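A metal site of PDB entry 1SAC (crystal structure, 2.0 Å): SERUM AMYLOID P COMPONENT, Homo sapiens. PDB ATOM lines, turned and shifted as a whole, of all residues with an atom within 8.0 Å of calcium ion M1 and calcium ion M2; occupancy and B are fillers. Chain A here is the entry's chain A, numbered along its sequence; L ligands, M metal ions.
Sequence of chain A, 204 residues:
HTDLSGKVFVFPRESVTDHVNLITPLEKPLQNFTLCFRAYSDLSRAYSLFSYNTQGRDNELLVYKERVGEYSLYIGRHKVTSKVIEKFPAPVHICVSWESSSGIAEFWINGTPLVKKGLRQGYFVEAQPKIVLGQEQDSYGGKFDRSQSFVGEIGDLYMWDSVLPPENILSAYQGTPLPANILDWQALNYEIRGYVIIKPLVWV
Calcium ion M1 is bound by OE1 of Glu 136 (2.4 Å).
OE1 of Gln 148 binds calcium ion M1 (2.6 Å).
An oxygen (O2) of the ligand binds calcium ion M1 (2.7 Å).
OD2 of Asp 138 binds calcium ion M1, 2.7 Å away.
OD1 of Asp 138 binds calcium ion M1 (2.8 Å).
Calcium ion M1 has five donor atoms within binding distance.
Of the 24 residues printed, 3 come within 4 Å of calcium ion M1.
The nearest printed residue that does not touch calcium ion M1 is Asp 145 (4.2 Å).
Calcium ion M2 is bound by the backbone carbonyl oxygen (O) of Gln 137 (2.5 Å), the side-chain amide oxygen (OD1) of Asn 59 (2.5 Å), the side-chain carboxylate (OD1) of Asp 138 (2.5 Å), the side-chain carboxylate (OE2) of Glu 136 (2.6 Å), the side-chain carboxylate (OD1) of Asp 58 (2.7 Å), an oxygen (O1) of the ligand (2.8 Å), the side-chain carboxylate (OD2) of Asp 58 (2.8 Å) and the side-chain carboxylate (OE1) of Glu 136 (2.8 Å).
ND2 of Asn 53 sits close to O of Gln 137.
O of Ser 51 is in hydrogen-bond range of NE2 of Gln 137, 3.1 Å away.
The side-chain amide oxygen of Gln 137 lies close to the backbone carbonyl oxygen of Ser 139 (3.4 Å).
N of Asn 59 lies within hydrogen-bond range of OD1 of Asn 53 (3.0 Å).
N of Asp 138 sits close to O of Lys 143 (3.4 Å).
OH of Tyr 64 lies within hydrogen-bond range of NE2 of Gln 148, 3.2 Å away.
O of Gln 148 is in hydrogen-bond range of N of Ser 48 (3.1 Å).
The backbone carbonyl oxygen (O) of Asp 58 is in hydrogen-bond range of the guanidinium group (NH1) of Arg 77 (2.6 Å).
Within 4 Å of calcium ion M2: Asp 58, Asn 59, Glu 136, Gln 137 and Asp 138.
The nearest printed residue that does not touch calcium ion M2 is Asn 53 (4.9 Å).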
ATOM      1  N   SER A  48      -5.514  25.057 -14.063  1.00  0.00           N
ATOM      2  CA  SER A  48      -6.157  25.924 -13.063  1.00  0.00           C
ATOM      3  C   SER A  48      -6.865  27.084 -13.751  1.00  0.00           C
ATOM      4  O   SER A  48      -6.273  27.716 -14.629  1.00  0.00           O
ATOM      5  CB  SER A  48      -5.089  26.467 -12.111  1.00  0.00           C
ATOM      6  OG  SER A  48      -5.700  27.123 -11.008  1.00  0.00           O
ATOM      7  N   SER A  51      -7.119  30.360  -8.698  1.00  0.00           N
ATOM      8  CA  SER A  51      -6.329  29.876  -7.563  1.00  0.00           C
ATOM      9  C   SER A  51      -6.429  30.878  -6.400  1.00  0.00           C
ATOM     10  O   SER A  51      -6.003  32.040  -6.535  1.00  0.00           O
ATOM     11  CB  SER A  51      -4.876  29.703  -7.978  1.00  0.00           C
ATOM     12  OG  SER A  51      -4.156  29.034  -6.960  1.00  0.00           O
ATOM     13  N   TYR A  52      -6.975  30.375  -5.317  1.00  0.00           N
ATOM     14  CA  TYR A  52      -7.279  31.124  -4.084  1.00  0.00           C
ATOM     15  C   TYR A  52      -6.686  30.381  -2.870  1.00  0.00           C
ATOM     16  O   TYR A  52      -7.310  29.449  -2.331  1.00  0.00           O
ATOM     17  CB  TYR A  52      -8.809  31.218  -3.987  1.00  0.00           C
ATOM     18  CG  TYR A  52      -9.361  31.980  -2.781  1.00  0.00           C
ATOM     19  CD1 TYR A  52      -9.042  31.561  -1.478  1.00  0.00           C
ATOM     20  CD2 TYR A  52     -10.203  33.083  -2.980  1.00  0.00           C
ATOM     21  CE1 TYR A  52      -9.576  32.255  -0.375  1.00  0.00           C
ATOM     22  CE2 TYR A  52     -10.728  33.766  -1.877  1.00  0.00           C
ATOM     23  CZ  TYR A  52     -10.419  33.357  -0.574  1.00  0.00           C
ATOM     24  OH  TYR A  52     -10.940  34.015   0.495  1.00  0.00           O
ATOM     25  N   ASN A  53      -5.498  30.811  -2.473  1.00  0.00           N
ATOM     26  CA  ASN A  53      -4.762  30.222  -1.342  1.00  0.00           C
ATOM     27  C   ASN A  53      -4.692  31.213  -0.171  1.00  0.00           C
ATOM     28  O   ASN A  53      -4.641  32.424  -0.364  1.00  0.00           O
ATOM     29  CB  ASN A  53      -3.325  29.876  -1.769  1.00  0.00           C
ATOM     30  CG  ASN A  53      -3.202  28.451  -2.343  1.00  0.00           C
ATOM     31  OD1 ASN A  53      -4.176  27.920  -2.872  1.00  0.00           O
ATOM     32  ND2 ASN A  53      -2.047  27.812  -2.262  1.00  0.00           N
ATOM     33  N   ARG A  57      -2.617  27.409   3.846  1.00  0.00           N
ATOM     34  CA  ARG A  57      -3.715  26.586   3.310  1.00  0.00           C
ATOM     35  C   ARG A  57      -3.690  26.544   1.801  1.00  0.00           C
ATOM     36  O   ARG A  57      -4.049  27.503   1.139  1.00  0.00           O
ATOM     37  CB  ARG A  57      -5.065  27.116   3.794  1.00  0.00           C
ATOM     38  CG  ARG A  57      -5.401  26.456   5.123  1.00  0.00           C
ATOM     39  CD  ARG A  57      -5.991  27.476   6.088  1.00  0.00           C
ATOM     40  NE  ARG A  57      -7.341  27.035   6.463  1.00  0.00           N
ATOM     41  CZ  ARG A  57      -7.813  27.168   7.712  1.00  0.00           C
ATOM     42  NH1 ARG A  57      -7.000  27.466   8.728  1.00  0.00           N
ATOM     43  NH2 ARG A  57      -9.117  27.005   7.934  1.00  0.00           N
ATOM     44  N   ASP A  58      -3.265  25.417   1.290  1.00  0.00           N
ATOM     45  CA  ASP A  58      -3.310  25.196  -0.173  1.00  0.00           C
ATOM     46  C   ASP A  58      -4.725  24.843  -0.606  1.00  0.00           C
ATOM     47  O   ASP A  58      -5.448  24.233   0.165  1.00  0.00           O
ATOM     48  CB  ASP A  58      -2.380  24.027  -0.529  1.00  0.00           C
ATOM     49  CG  ASP A  58      -2.211  23.939  -2.045  1.00  0.00           C
ATOM     50  OD1 ASP A  58      -2.312  25.003  -2.684  1.00  0.00           O
ATOM     51  OD2 ASP A  58      -1.976  22.833  -2.541  1.00  0.00           O
ATOM     52  N   ASN A  59      -5.150  25.271  -1.767  1.00  0.00           N
ATOM     53  CA  ASN A  59      -6.407  24.810  -2.361  1.00  0.00           C
ATOM     54  C   ASN A  59      -7.573  25.151  -1.438  1.00  0.00           C
ATOM     55  O   ASN A  59      -8.473  24.323  -1.225  1.00  0.00           O
ATOM     56  CB  ASN A  59      -6.351  23.299  -2.582  1.00  0.00           C
ATOM     57  CG  ASN A  59      -5.376  22.963  -3.703  1.00  0.00           C
ATOM     58  OD1 ASN A  59      -4.821  23.878  -4.310  1.00  0.00           O
ATOM     59  ND2 ASN A  59      -5.141  21.712  -4.014  1.00  0.00           N
ATOM     60  N   GLU A  60      -7.557  26.370  -1.041  1.00  0.00           N
ATOM     61  CA  GLU A  60      -8.583  26.921  -0.149  1.00  0.00           C
ATOM     62  C   GLU A  60      -9.902  27.140  -0.928  1.00  0.00           C
ATOM     63  O   GLU A  60     -10.998  26.905  -0.418  1.00  0.00           O
ATOM     64  CB  GLU A  60      -8.101  28.247   0.445  1.00  0.00           C
ATOM     65  CG  GLU A  60      -9.036  28.803   1.511  1.00  0.00           C
ATOM     66  CD  GLU A  60      -9.254  27.847   2.682  1.00  0.00           C
ATOM     67  OE1 GLU A  60      -8.613  26.728   2.736  1.00  0.00           O
ATOM     68  OE2 GLU A  60     -10.077  28.149   3.622  1.00  0.00           O
ATOM     69  N   LEU A  62     -10.278  26.662  -5.195  1.00  0.00           N
ATOM     70  CA  LEU A  62      -9.632  26.413  -6.504  1.00  0.00           C
ATOM     71  C   LEU A  62     -10.638  25.854  -7.506  1.00  0.00           C
ATOM     72  O   LEU A  62     -11.359  24.893  -7.210  1.00  0.00           O
ATOM     73  CB  LEU A  62      -8.476  25.413  -6.303  1.00  0.00           C
ATOM     74  CG  LEU A  62      -7.972  24.764  -7.600  1.00  0.00           C
ATOM     75  CD1 LEU A  62      -7.196  25.738  -8.492  1.00  0.00           C
ATOM     76  CD2 LEU A  62      -7.026  23.584  -7.349  1.00  0.00           C
ATOM     77  N   TYR A  64     -10.805  24.178 -11.048  1.00  0.00           N
ATOM     78  CA  TYR A  64      -9.796  23.388 -11.801  1.00  0.00           C
ATOM     79  C   TYR A  64     -10.512  22.662 -12.952  1.00  0.00           C
ATOM     80  O   TYR A  64     -11.634  22.210 -12.690  1.00  0.00           O
ATOM     81  CB  TYR A  64      -9.160  22.379 -10.882  1.00  0.00           C
ATOM     82  CG  TYR A  64      -7.861  21.779 -11.396  1.00  0.00           C
ATOM     83  CD1 TYR A  64      -6.683  22.527 -11.357  1.00  0.00           C
ATOM     84  CD2 TYR A  64      -7.847  20.482 -11.883  1.00  0.00           C
ATOM     85  CE1 TYR A  64      -5.496  21.964 -11.824  1.00  0.00           C
ATOM     86  CE2 TYR A  64      -6.664  19.925 -12.343  1.00  0.00           C
ATOM     87  CZ  TYR A  64      -5.478  20.662 -12.318  1.00  0.00           C
ATOM     88  OH  TYR A  64      -4.289  20.130 -12.767  1.00  0.00           O
ATOM     89  N   TYR A  74     -12.547  23.008  -5.436  1.00  0.00           N
ATOM     90  CA  TYR A  74     -11.921  22.694  -4.139  1.00  0.00           C
ATOM     91  C   TYR A  74     -12.301  23.751  -3.097  1.00  0.00           C
ATOM     92  O   TYR A  74     -12.131  24.951  -3.311  1.00  0.00           O
ATOM     93  CB  TYR A  74     -10.391  22.778  -4.210  1.00  0.00           C
ATOM     94  CG  TYR A  74      -9.681  21.600  -4.895  1.00  0.00           C
ATOM     95  CD1 TYR A  74      -9.698  21.494  -6.293  1.00  0.00           C
ATOM     96  CD2 TYR A  74      -9.007  20.633  -4.129  1.00  0.00           C
ATOM     97  CE1 TYR A  74      -9.030  20.442  -6.921  1.00  0.00           C
ATOM     98  CE2 TYR A  74      -8.327  19.582  -4.765  1.00  0.00           C
ATOM     99  CZ  TYR A  74      -8.341  19.489  -6.158  1.00  0.00           C
ATOM    100  OH  TYR A  74      -7.670  18.479  -6.775  1.00  0.00           O
ATOM    101  N   ARG A  77      -9.600  22.260   0.544  1.00  0.00           N
ATOM    102  CA  ARG A  77      -8.808  21.065   0.157  1.00  0.00           C
ATOM    103  C   ARG A  77      -9.696  19.846  -0.181  1.00  0.00           C
ATOM    104  O   ARG A  77      -9.200  18.797  -0.601  1.00  0.00           O
ATOM    105  CB  ARG A  77      -7.867  20.670   1.280  1.00  0.00           C
ATOM    106  CG  ARG A  77      -6.504  21.356   1.165  1.00  0.00           C
ATOM    107  CD  ARG A  77      -5.902  21.725   2.522  1.00  0.00           C
ATOM    108  NE  ARG A  77      -6.880  22.322   3.447  1.00  0.00           N
ATOM    109  CZ  ARG A  77      -7.363  23.569   3.324  1.00  0.00           C
ATOM    110  NH1 ARG A  77      -6.979  24.367   2.320  1.00  0.00           N
ATOM    111  NH2 ARG A  77      -8.252  24.117   4.171  1.00  0.00           N
ATOM    112  N   GLN A 135      -1.565  30.646 -13.207  1.00  0.00           N
ATOM    113  CA  GLN A 135      -0.875  29.528 -12.536  1.00  0.00           C
ATOM    114  C   GLN A 135      -1.726  29.020 -11.372  1.00  0.00           C
ATOM    115  O   GLN A 135      -2.590  29.742 -10.860  1.00  0.00           O
ATOM    116  CB  GLN A 135       0.475  30.003 -11.984  1.00  0.00           C
ATOM    117  CG  GLN A 135       1.349  30.670 -13.037  1.00  0.00           C
ATOM    118  CD  GLN A 135       1.915  29.688 -14.074  1.00  0.00           C
ATOM    119  OE1 GLN A 135       2.010  28.490 -13.807  1.00  0.00           O
ATOM    120  NE2 GLN A 135       2.298  30.131 -15.260  1.00  0.00           N
ATOM    121  N   GLU A 136      -1.278  27.878 -10.933  1.00  0.00           N
ATOM    122  CA  GLU A 136      -1.804  27.174  -9.762  1.00  0.00           C
ATOM    123  C   GLU A 136      -0.796  27.263  -8.608  1.00  0.00           C
ATOM    124  O   GLU A 136       0.396  26.935  -8.769  1.00  0.00           O
ATOM    125  CB  GLU A 136      -2.059  25.717 -10.121  1.00  0.00           C
ATOM    126  CG  GLU A 136      -3.267  25.137  -9.399  1.00  0.00           C
ATOM    127  CD  GLU A 136      -2.917  24.696  -7.991  1.00  0.00           C
ATOM    128  OE1 GLU A 136      -1.829  24.036  -7.792  1.00  0.00           O
ATOM    129  OE2 GLU A 136      -3.698  24.979  -7.011  1.00  0.00           O
ATOM    130  N   GLN A 137      -1.220  27.806  -7.490  1.00  0.00           N
ATOM    131  CA  GLN A 137      -0.408  27.989  -6.285  1.00  0.00           C
ATOM    132  C   GLN A 137      -0.385  26.741  -5.403  1.00  0.00           C
ATOM    133  O   GLN A 137      -1.411  26.078  -5.211  1.00  0.00           O
ATOM    134  CB  GLN A 137      -1.006  29.051  -5.359  1.00  0.00           C
ATOM    135  CG  GLN A 137      -1.202  30.429  -5.981  1.00  0.00           C
ATOM    136  CD  GLN A 137      -1.948  31.385  -5.041  1.00  0.00           C
ATOM    137  OE1 GLN A 137      -1.353  31.887  -4.089  1.00  0.00           O
ATOM    138  NE2 GLN A 137      -3.219  31.655  -5.244  1.00  0.00           N
ATOM    139  N   ASP A 138       0.814  26.422  -4.907  1.00  0.00           N
ATOM    140  CA  ASP A 138       0.973  25.366  -3.903  1.00  0.00           C
ATOM    141  C   ASP A 138       1.388  25.976  -2.567  1.00  0.00           C
ATOM    142  O   ASP A 138       1.350  25.312  -1.526  1.00  0.00           O
ATOM    143  CB  ASP A 138       2.020  24.355  -4.375  1.00  0.00           C
ATOM    144  CG  ASP A 138       1.300  23.299  -5.222  1.00  0.00           C
ATOM    145  OD1 ASP A 138       0.020  23.214  -5.190  1.00  0.00           O
ATOM    146  OD2 ASP A 138       1.988  22.488  -5.961  1.00  0.00           O
ATOM    147  N   SER A 139       1.766  27.240  -2.656  1.00  0.00           N
ATOM    148  CA  SER A 139       2.172  28.036  -1.487  1.00  0.00           C
ATOM    149  C   SER A 139       1.473  29.386  -1.535  1.00  0.00           C
ATOM    150  O   SER A 139       0.582  29.622  -2.377  1.00  0.00           O
ATOM    151  CB  SER A 139       3.689  28.235  -1.489  1.00  0.00           C
ATOM    152  OG  SER A 139       4.091  28.935  -2.658  1.00  0.00           O
ATOM    153  N   GLY A 142       2.819  31.349  -4.389  1.00  0.00           N
ATOM    154  CA  GLY A 142       3.855  30.838  -5.307  1.00  0.00           C
ATOM    155  C   GLY A 142       3.738  29.325  -5.485  1.00  0.00           C
ATOM    156  O   GLY A 142       2.634  28.806  -5.383  1.00  0.00           O
ATOM    157  N   LYS A 143       4.861  28.691  -5.723  1.00  0.00           N
ATOM    158  CA  LYS A 143       5.049  27.272  -5.969  1.00  0.00           C
ATOM    159  C   LYS A 143       4.201  26.804  -7.136  1.00  0.00           C
ATOM    160  O   LYS A 143       3.418  25.875  -6.985  1.00  0.00           O
ATOM    161  CB  LYS A 143       4.755  26.448  -4.738  1.00  0.00           C
ATOM    162  CG  LYS A 143       6.039  25.891  -4.158  1.00  0.00           C
ATOM    163  CD  LYS A 143       5.939  25.838  -2.644  1.00  0.00           C
ATOM    164  CE  LYS A 143       5.290  24.536  -2.203  1.00  0.00           C
ATOM    165  NZ  LYS A 143       4.905  24.620  -0.781  1.00  0.00           N
ATOM    166  N   PHE A 144       4.334  27.427  -8.257  1.00  0.00           N
ATOM    167  CA  PHE A 144       3.533  27.135  -9.453  1.00  0.00           C
ATOM    168  C   PHE A 144       4.044  25.808 -10.092  1.00  0.00           C
ATOM    169  O   PHE A 144       5.142  25.334  -9.783  1.00  0.00           O
ATOM    170  CB  PHE A 144       3.656  28.312 -10.446  1.00  0.00           C
ATOM    171  CG  PHE A 144       3.191  29.655  -9.850  1.00  0.00           C
ATOM    172  CD1 PHE A 144       2.108  29.691  -8.959  1.00  0.00           C
ATOM    173  CD2 PHE A 144       3.855  30.851 -10.183  1.00  0.00           C
ATOM    174  CE1 PHE A 144       1.684  30.909  -8.421  1.00  0.00           C
ATOM    175  CE2 PHE A 144       3.434  32.069  -9.631  1.00  0.00           C
ATOM    176  CZ  PHE A 144       2.349  32.104  -8.754  1.00  0.00           C
ATOM    177  N   ASP A 145       3.194  25.210 -10.945  1.00  0.00           N
ATOM    178  CA  ASP A 145       3.516  23.958 -11.711  1.00  0.00           C
ATOM    179  C   ASP A 145       3.106  24.162 -13.175  1.00  0.00           C
ATOM    180  O   ASP A 145       1.963  24.571 -13.457  1.00  0.00           O
ATOM    181  CB  ASP A 145       2.729  22.754 -11.133  1.00  0.00           C
ATOM    182  CG  ASP A 145       2.850  21.413 -11.915  1.00  0.00           C
ATOM    183  OD1 ASP A 145       3.515  21.347 -13.023  1.00  0.00           O
ATOM    184  OD2 ASP A 145       2.287  20.345 -11.457  1.00  0.00           O
ATOM    185  N   ARG A 146       4.106  24.221 -14.007  1.00  0.00           N
ATOM    186  CA  ARG A 146       3.924  24.431 -15.443  1.00  0.00           C
ATOM    187  C   ARG A 146       2.838  23.541 -16.032  1.00  0.00           C
ATOM    188  O   ARG A 146       2.184  23.907 -17.022  1.00  0.00           O
ATOM    189  CB  ARG A 146       5.218  24.160 -16.181  1.00  0.00           C
ATOM    190  CG  ARG A 146       5.041  24.237 -17.676  1.00  0.00           C
ATOM    191  CD  ARG A 146       6.293  23.796 -18.400  1.00  0.00           C
ATOM    192  NE  ARG A 146       7.290  24.846 -18.467  1.00  0.00           N
ATOM    193  CZ  ARG A 146       7.431  25.633 -19.519  1.00  0.00           C
ATOM    194  NH1 ARG A 146       6.647  25.465 -20.593  1.00  0.00           N
ATOM    195  NH2 ARG A 146       8.334  26.619 -19.589  1.00  0.00           N
ATOM    196  N   SER A 147       2.600  22.346 -15.580  1.00  0.00           N
ATOM    197  CA  SER A 147       1.598  21.441 -16.178  1.00  0.00           C
ATOM    198  C   SER A 147       0.209  21.762 -15.648  1.00  0.00           C
ATOM    199  O   SER A 147      -0.779  21.079 -15.895  1.00  0.00           O
ATOM    200  CB  SER A 147       1.959  19.988 -15.863  1.00  0.00           C
ATOM    201  OG  SER A 147       1.802  19.782 -14.456  1.00  0.00           O
ATOM    202  N   GLN A 148       0.106  22.854 -14.937  1.00  0.00           N
ATOM    203  CA  GLN A 148      -1.218  23.292 -14.491  1.00  0.00           C
ATOM    204  C   GLN A 148      -1.484  24.723 -14.930  1.00  0.00           C
ATOM    205  O   GLN A 148      -2.446  25.370 -14.485  1.00  0.00           O
ATOM    206  CB  GLN A 148      -1.298  23.248 -12.973  1.00  0.00           C
ATOM    207  CG  GLN A 148      -1.175  21.831 -12.403  1.00  0.00           C
ATOM    208  CD  GLN A 148      -1.495  21.819 -10.923  1.00  0.00           C
ATOM    209  OE1 GLN A 148      -1.066  22.711 -10.195  1.00  0.00           O
ATOM    210  NE2 GLN A 148      -2.268  20.870 -10.428  1.00  0.00           N
HETATM  211  C1  LIG L   1      -2.832  21.077  -6.920  1.00  0.00           C
HETATM  212  O1  LIG L   1      -2.620  21.132  -5.706  1.00  0.00           O
HETATM  213  O2  LIG L   1      -1.868  20.848  -7.670  1.00  0.00           O
HETATM  214  C2  LIG L   1      -4.255  20.776  -7.414  1.00  0.00           C
HETATM  215 CA    CA M   1       0.111  22.626  -7.894  1.00  0.00          CA
HETATM  216 CA    CA M   2      -2.434  23.807  -5.082  1.00  0.00          CA
